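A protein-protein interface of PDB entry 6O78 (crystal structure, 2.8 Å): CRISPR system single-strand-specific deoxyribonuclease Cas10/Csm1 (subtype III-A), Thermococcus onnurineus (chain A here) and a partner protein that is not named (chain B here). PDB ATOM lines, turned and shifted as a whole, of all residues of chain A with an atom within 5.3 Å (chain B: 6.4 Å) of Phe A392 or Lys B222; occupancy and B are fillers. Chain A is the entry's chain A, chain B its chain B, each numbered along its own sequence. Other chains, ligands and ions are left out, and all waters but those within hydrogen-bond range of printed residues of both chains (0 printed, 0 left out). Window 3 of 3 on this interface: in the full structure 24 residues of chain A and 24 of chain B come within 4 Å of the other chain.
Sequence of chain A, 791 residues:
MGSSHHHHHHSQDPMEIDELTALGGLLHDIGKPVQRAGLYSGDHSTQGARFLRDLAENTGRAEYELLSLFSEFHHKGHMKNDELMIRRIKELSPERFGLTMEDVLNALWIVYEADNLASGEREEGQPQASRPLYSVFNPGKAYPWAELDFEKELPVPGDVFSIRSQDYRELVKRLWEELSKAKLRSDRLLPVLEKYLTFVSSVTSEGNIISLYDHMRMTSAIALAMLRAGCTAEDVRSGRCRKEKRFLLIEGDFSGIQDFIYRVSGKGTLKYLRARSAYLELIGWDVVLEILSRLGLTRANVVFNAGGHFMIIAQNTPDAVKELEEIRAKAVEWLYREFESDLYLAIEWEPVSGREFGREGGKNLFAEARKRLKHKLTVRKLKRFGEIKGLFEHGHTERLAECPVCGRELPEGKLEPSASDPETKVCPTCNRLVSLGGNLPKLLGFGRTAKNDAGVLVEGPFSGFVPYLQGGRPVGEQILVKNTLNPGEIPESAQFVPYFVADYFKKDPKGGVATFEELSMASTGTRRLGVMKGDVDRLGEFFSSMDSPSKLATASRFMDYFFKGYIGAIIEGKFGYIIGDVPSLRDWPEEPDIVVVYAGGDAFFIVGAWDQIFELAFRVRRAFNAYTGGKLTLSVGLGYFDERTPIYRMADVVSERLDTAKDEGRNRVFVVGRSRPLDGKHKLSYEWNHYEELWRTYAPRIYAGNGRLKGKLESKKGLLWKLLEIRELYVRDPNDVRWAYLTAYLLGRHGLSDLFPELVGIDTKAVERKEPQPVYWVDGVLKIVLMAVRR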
ATOM      1  N   PHE A 385      16.522  10.107 -27.880  1.00  0.00           N
ATOM      2  CA  PHE A 385      17.628  10.867 -27.241  1.00  0.00           C
ATOM      3  C   PHE A 385      17.210  11.328 -25.838  1.00  0.00           C
ATOM      4  O   PHE A 385      17.696  12.383 -25.381  1.00  0.00           O
ATOM      5  CB  PHE A 385      18.058  12.036 -28.131  1.00  0.00           C
ATOM      6  CG  PHE A 385      18.538  11.629 -29.500  1.00  0.00           C
ATOM      7  CD1 PHE A 385      19.803  11.092 -29.676  1.00  0.00           C
ATOM      8  CD2 PHE A 385      17.726  11.781 -30.614  1.00  0.00           C
ATOM      9  CE1 PHE A 385      20.246  10.716 -30.934  1.00  0.00           C
ATOM     10  CE2 PHE A 385      18.171  11.405 -31.873  1.00  0.00           C
ATOM     11  CZ  PHE A 385      19.430  10.874 -32.029  1.00  0.00           C
ATOM     12  N   GLY A 386      16.354  10.545 -25.167  1.00  0.00           N
ATOM     13  CA  GLY A 386      16.041  10.696 -23.733  1.00  0.00           C
ATOM     14  C   GLY A 386      17.256  10.395 -22.870  1.00  0.00           C
ATOM     15  O   GLY A 386      17.273  10.832 -21.702  1.00  0.00           O
ATOM     16  N   ILE A 388      20.065  11.670 -23.402  1.00  0.00           N
ATOM     17  CA  ILE A 388      20.841  12.945 -23.495  1.00  0.00           C
ATOM     18  C   ILE A 388      20.022  14.051 -22.817  1.00  0.00           C
ATOM     19  O   ILE A 388      18.981  14.440 -23.382  1.00  0.00           O
ATOM     20  CB  ILE A 388      21.161  13.274 -24.970  1.00  0.00           C
ATOM     21  CG1 ILE A 388      22.152  12.271 -25.566  1.00  0.00           C
ATOM     22  CG2 ILE A 388      21.660  14.705 -25.125  1.00  0.00           C
ATOM     23  CD1 ILE A 388      22.200  12.282 -27.073  1.00  0.00           C
ATOM     24  N   LYS A 389      20.479  14.536 -21.656  1.00  0.00           N
ATOM     25  CA  LYS A 389      19.729  15.494 -20.796  1.00  0.00           C
ATOM     26  C   LYS A 389      19.902  16.927 -21.315  1.00  0.00           C
ATOM     27  O   LYS A 389      18.924  17.699 -21.235  1.00  0.00           O
ATOM     28  CB  LYS A 389      20.188  15.393 -19.338  1.00  0.00           C
ATOM     29  CG  LYS A 389      19.278  16.100 -18.342  1.00  0.00           C
ATOM     30  CD  LYS A 389      19.049  15.323 -17.064  1.00  0.00           C
ATOM     31  CE  LYS A 389      18.182  14.097 -17.258  1.00  0.00           C
ATOM     32  NZ  LYS A 389      18.070  13.307 -16.010  1.00  0.00           N
ATOM     33  N   GLY A 390      21.092  17.265 -21.825  1.00  0.00           N
ATOM     34  CA  GLY A 390      21.409  18.582 -22.412  1.00  0.00           C
ATOM     35  C   GLY A 390      20.516  18.922 -23.598  1.00  0.00           C
ATOM     36  O   GLY A 390      20.528  20.097 -24.019  1.00  0.00           O
ATOM     37  N   LEU A 391      19.778  17.935 -24.118  1.00  0.00           N
ATOM     38  CA  LEU A 391      18.861  18.055 -25.286  1.00  0.00           C
ATOM     39  C   LEU A 391      17.839  19.176 -25.055  1.00  0.00           C
ATOM     40  O   LEU A 391      17.632  19.978 -25.986  1.00  0.00           O
ATOM     41  CB  LEU A 391      18.162  16.707 -25.499  1.00  0.00           C
ATOM     42  CG  LEU A 391      17.164  16.640 -26.654  1.00  0.00           C
ATOM     43  CD1 LEU A 391      17.812  17.042 -27.970  1.00  0.00           C
ATOM     44  CD2 LEU A 391      16.566  15.246 -26.765  1.00  0.00           C
ATOM     45  N   PHE A 392      17.232  19.227 -23.863  1.00  0.00           N
ATOM     46  CA  PHE A 392      16.088  20.114 -23.521  1.00  0.00           C
ATOM     47  C   PHE A 392      16.587  21.356 -22.770  1.00  0.00           C
ATOM     48  O   PHE A 392      16.050  21.661 -21.684  1.00  0.00           O
ATOM     49  CB  PHE A 392      15.046  19.332 -22.716  1.00  0.00           C
ATOM     50  CG  PHE A 392      14.595  18.049 -23.368  1.00  0.00           C
ATOM     51  CD1 PHE A 392      14.047  18.056 -24.642  1.00  0.00           C
ATOM     52  CD2 PHE A 392      14.720  16.834 -22.713  1.00  0.00           C
ATOM     53  CE1 PHE A 392      13.631  16.878 -25.243  1.00  0.00           C
ATOM     54  CE2 PHE A 392      14.306  15.656 -23.316  1.00  0.00           C
ATOM     55  CZ  PHE A 392      13.760  15.680 -24.579  1.00  0.00           C
ATOM     56  N   GLU A 393      17.568  22.058 -23.352  1.00  0.00           N
ATOM     57  CA  GLU A 393      18.188  23.294 -22.797  1.00  0.00           C
ATOM     58  C   GLU A 393      18.642  24.195 -23.953  1.00  0.00           C
ATOM     59  O   GLU A 393      18.536  25.427 -23.789  1.00  0.00           O
ATOM     60  CB  GLU A 393      19.362  22.935 -21.883  1.00  0.00           C
ATOM     61  CG  GLU A 393      18.947  22.588 -20.463  1.00  0.00           C
ATOM     62  CD  GLU A 393      19.843  21.580 -19.764  1.00  0.00           C
ATOM     63  OE1 GLU A 393      21.077  21.670 -19.927  1.00  0.00           O
ATOM     64  OE2 GLU A 393      19.303  20.702 -19.062  1.00  0.00           O
ATOM     65  N   PRO B 220      10.570  22.116 -24.312  1.00  0.00           N
ATOM     66  CA  PRO B 220      10.303  21.639 -22.954  1.00  0.00           C
ATOM     67  C   PRO B 220      11.330  22.125 -21.923  1.00  0.00           C
ATOM     68  O   PRO B 220      12.450  22.419 -22.302  1.00  0.00           O
ATOM     69  CB  PRO B 220      10.379  20.115 -23.113  1.00  0.00           C
ATOM     70  CG  PRO B 220      11.399  19.931 -24.216  1.00  0.00           C
ATOM     71  CD  PRO B 220      11.120  21.064 -25.182  1.00  0.00           C
ATOM     72  N   THR B 221      10.915  22.187 -20.654  1.00  0.00           N
ATOM     73  CA  THR B 221      11.730  22.627 -19.487  1.00  0.00           C
ATOM     74  C   THR B 221      12.157  21.395 -18.680  1.00  0.00           C
ATOM     75  O   THR B 221      13.330  21.345 -18.264  1.00  0.00           O
ATOM     76  CB  THR B 221      10.954  23.645 -18.641  1.00  0.00           C
ATOM     77  OG1 THR B 221       9.868  22.978 -17.997  1.00  0.00           O
ATOM     78  CG2 THR B 221      10.422  24.800 -19.463  1.00  0.00           C
ATOM     79  N   LYS B 222      11.235  20.448 -18.474  1.00  0.00           N
ATOM     80  CA  LYS B 222      11.509  19.103 -17.898  1.00  0.00           C
ATOM     81  C   LYS B 222      11.972  18.180 -19.030  1.00  0.00           C
ATOM     82  O   LYS B 222      12.292  18.695 -20.120  1.00  0.00           O
ATOM     83  CB  LYS B 222      10.257  18.522 -17.227  1.00  0.00           C
ATOM     84  CG  LYS B 222       9.406  19.516 -16.449  1.00  0.00           C
ATOM     85  CD  LYS B 222       8.535  18.882 -15.383  1.00  0.00           C
ATOM     86  CE  LYS B 222       8.196  19.841 -14.261  1.00  0.00           C
ATOM     87  NZ  LYS B 222       7.540  19.149 -13.126  1.00  0.00           N
ATOM     88  N   THR B 223      12.007  16.869 -18.778  1.00  0.00           N
ATOM     89  CA  THR B 223      12.082  15.811 -19.819  1.00  0.00           C
ATOM     90  C   THR B 223      10.679  15.233 -19.989  1.00  0.00           C
ATOM     91  O   THR B 223      10.056  14.831 -19.009  1.00  0.00           O
ATOM     92  CB  THR B 223      13.124  14.742 -19.463  1.00  0.00           C
ATOM     93  OG1 THR B 223      12.633  13.990 -18.353  1.00  0.00           O
ATOM     94  CG2 THR B 223      14.480  15.323 -19.125  1.00  0.00           C
ATOM     95  N   PRO B 224      10.130  15.186 -21.224  1.00  0.00           N
ATOM     96  CA  PRO B 224       8.746  14.751 -21.432  1.00  0.00           C
ATOM     97  C   PRO B 224       8.563  13.238 -21.236  1.00  0.00           C
ATOM     98  O   PRO B 224       9.531  12.566 -20.919  1.00  0.00           O
ATOM     99  CB  PRO B 224       8.486  15.170 -22.886  1.00  0.00           C
ATOM    100  CG  PRO B 224       9.840  15.030 -23.534  1.00  0.00           C
ATOM    101  CD  PRO B 224      10.810  15.525 -22.484  1.00  0.00           C
ATOM    102  N   TRP B 227       7.367  11.363 -26.913  1.00  0.00           N
ATOM    103  CA  TRP B 227       7.617  12.484 -27.859  1.00  0.00           C
ATOM    104  C   TRP B 227       8.225  12.004 -29.181  1.00  0.00           C
ATOM    105  O   TRP B 227       8.822  10.911 -29.216  1.00  0.00           O
ATOM    106  CB  TRP B 227       8.501  13.546 -27.196  1.00  0.00           C
ATOM    107  CG  TRP B 227       9.955  13.194 -27.085  1.00  0.00           C
ATOM    108  CD1 TRP B 227      10.933  13.460 -27.999  1.00  0.00           C
ATOM    109  CD2 TRP B 227      10.610  12.546 -25.978  1.00  0.00           C
ATOM    110  NE1 TRP B 227      12.144  13.011 -27.546  1.00  0.00           N
ATOM    111  CE2 TRP B 227      11.979  12.449 -26.308  1.00  0.00           C
ATOM    112  CE3 TRP B 227      10.177  12.030 -24.750  1.00  0.00           C
ATOM    113  CZ2 TRP B 227      12.911  11.865 -25.450  1.00  0.00           C
ATOM    114  CZ3 TRP B 227      11.100  11.458 -23.901  1.00  0.00           C
ATOM    115  CH2 TRP B 227      12.448  11.375 -24.250  1.00  0.00           C
ATOM    116  N   LEU B 229      10.847  14.216 -31.864  1.00  0.00           N
ATOM    117  CA  LEU B 229      11.650  15.463 -31.994  1.00  0.00           C
ATOM    118  C   LEU B 229      11.344  16.127 -33.340  1.00  0.00           C
ATOM    119  O   LEU B 229      10.979  15.413 -34.292  1.00  0.00           O
ATOM    120  CB  LEU B 229      13.141  15.141 -31.863  1.00  0.00           C
ATOM    121  CG  LEU B 229      13.611  14.732 -30.467  1.00  0.00           C
ATOM    122  CD1 LEU B 229      15.087  14.372 -30.484  1.00  0.00           C
ATOM    123  CD2 LEU B 229      13.347  15.830 -29.448  1.00  0.00           C
ATOM    124  N   THR B 245      15.444  22.584 -31.267  1.00  0.00           N
ATOM    125  CA  THR B 245      14.853  21.220 -31.206  1.00  0.00           C
ATOM    126  C   THR B 245      13.544  21.299 -30.415  1.00  0.00           C
ATOM    127  O   THR B 245      13.607  21.461 -29.179  1.00  0.00           O
ATOM    128  CB  THR B 245      15.826  20.200 -30.600  1.00  0.00           C
ATOM    129  OG1 THR B 245      16.255  20.686 -29.327  1.00  0.00           O
ATOM    130  CG2 THR B 245      17.029  19.940 -31.481  1.00  0.00           C
ATOM    131  N   ILE B 247       9.669  19.689 -29.274  1.00  0.00           N
ATOM    132  CA  ILE B 247       8.781  18.506 -29.091  1.00  0.00           C
ATOM    133  C   ILE B 247       7.607  18.672 -30.060  1.00  0.00           C
ATOM    134  O   ILE B 247       7.017  19.765 -30.071  1.00  0.00           O
ATOM    135  CB  ILE B 247       8.314  18.404 -27.626  1.00  0.00           C
ATOM    136  CG1 ILE B 247       9.395  17.807 -26.724  1.00  0.00           C
ATOM    137  CG2 ILE B 247       7.021  17.619 -27.522  1.00  0.00           C
ATOM    138  CD1 ILE B 247       9.032  17.834 -25.261  1.00  0.00           C
ATOM    139  N   LYS B 254       4.304  16.037 -18.353  1.00  0.00           N
ATOM    140  CA  LYS B 254       3.779  16.046 -16.959  1.00  0.00           C
ATOM    141  C   LYS B 254       4.035  17.428 -16.343  1.00  0.00           C
ATOM    142  O   LYS B 254       5.124  17.635 -15.762  1.00  0.00           O
ATOM    143  CB  LYS B 254       4.397  14.914 -16.131  1.00  0.00           C
ATOM    144  CG  LYS B 254       3.538  14.444 -14.963  1.00  0.00           C
ATOM    145  CD  LYS B 254       4.204  13.418 -14.067  1.00  0.00           C
ATOM    146  CE  LYS B 254       5.186  14.028 -13.088  1.00  0.00           C
ATOM    147  NZ  LYS B 254       5.646  13.037 -12.087  1.00  0.00           N
ATOM    148  N   ASN B 255       3.060  18.333 -16.484  1.00  0.00           N
ATOM    149  CA  ASN B 255       3.086  19.721 -15.946  1.00  0.00           C
ATOM    150  C   ASN B 255       4.300  20.460 -16.522  1.00  0.00           C
ATOM    151  O   ASN B 255       5.151  20.925 -15.733  1.00  0.00           O
ATOM    152  CB  ASN B 255       3.071  19.733 -14.414  1.00  0.00           C
ATOM    153  CG  ASN B 255       2.960  21.127 -13.833  1.00  0.00           C
ATOM    154  OD1 ASN B 255       2.161  21.938 -14.298  1.00  0.00           O
ATOM    155  ND2 ASN B 255       3.760  21.417 -12.820  1.00  0.00           N
ATOM    156  N   ASP B 256       4.379  20.540 -17.854  1.00  0.00           N
ATOM    157  CA  ASP B 256       5.399  21.326 -18.596  1.00  0.00           C
ATOM    158  C   ASP B 256       4.681  22.461 -19.319  1.00  0.00           C
ATOM    159  O   ASP B 256       3.890  22.211 -20.224  1.00  0.00           O
ATOM    160  CB  ASP B 256       6.189  20.442 -19.564  1.00  0.00           C
ATOM    161  CG  ASP B 256       7.488  21.061 -20.055  1.00  0.00           C
ATOM    162  OD1 ASP B 256       7.671  22.282 -19.864  1.00  0.00           O
ATOM    163  OD2 ASP B 256       8.312  20.315 -20.624  1.00  0.00           O
ATOM    164  N   PRO B 257       4.914  23.738 -18.937  1.00  0.00           N
ATOM    165  CA  PRO B 257       4.300  24.868 -19.632  1.00  0.00           C
ATOM    166  C   PRO B 257       5.023  25.208 -20.945  1.00  0.00           C
ATOM    167  O   PRO B 257       4.541  26.057 -21.672  1.00  0.00           O
ATOM    168  CB  PRO B 257       4.463  26.010 -18.621  1.00  0.00           C
ATOM    169  CG  PRO B 257       5.763  25.683 -17.920  1.00  0.00           C
ATOM    170  CD  PRO B 257       5.784  24.171 -17.831  1.00  0.00           C
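Of the printed residues of chain B, Phe A385 touches Leu B229. Of the printed residues of chain B, Phe A392 touches Pro B220, Lys B222, Thr B223 and Pro B224. Printed residues of chain A within 4 Å of Pro B220: Phe A392. Lys B222 touches one residue of chain A. Of the printed residues of chain A, Thr B245 touches Leu A391 (3.7 Å).
Among the printed residues, pairs that only touch across the chains: Phe A392 with Pro B220 (3.3 Å), Phe A392 with Pro B224 (3.6 Å), Leu A391 with Thr B245 (3.7 Å), Gly A386 with Trp B227 (3.7 Å), Phe A385 with Leu B229 (3.7 Å), Phe A392 with Lys B222 (3.8 Å) and Phe A392 with Thr B223 (3.9 Å).
Of the 8 printed residues of chain A, 4 touch a printed residue of chain B. Hydrophobic or aromatic side chains of chain B within 4 Å of the printed part of chain A: Pro B220, Pro B224, Trp B227 and Leu B229.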
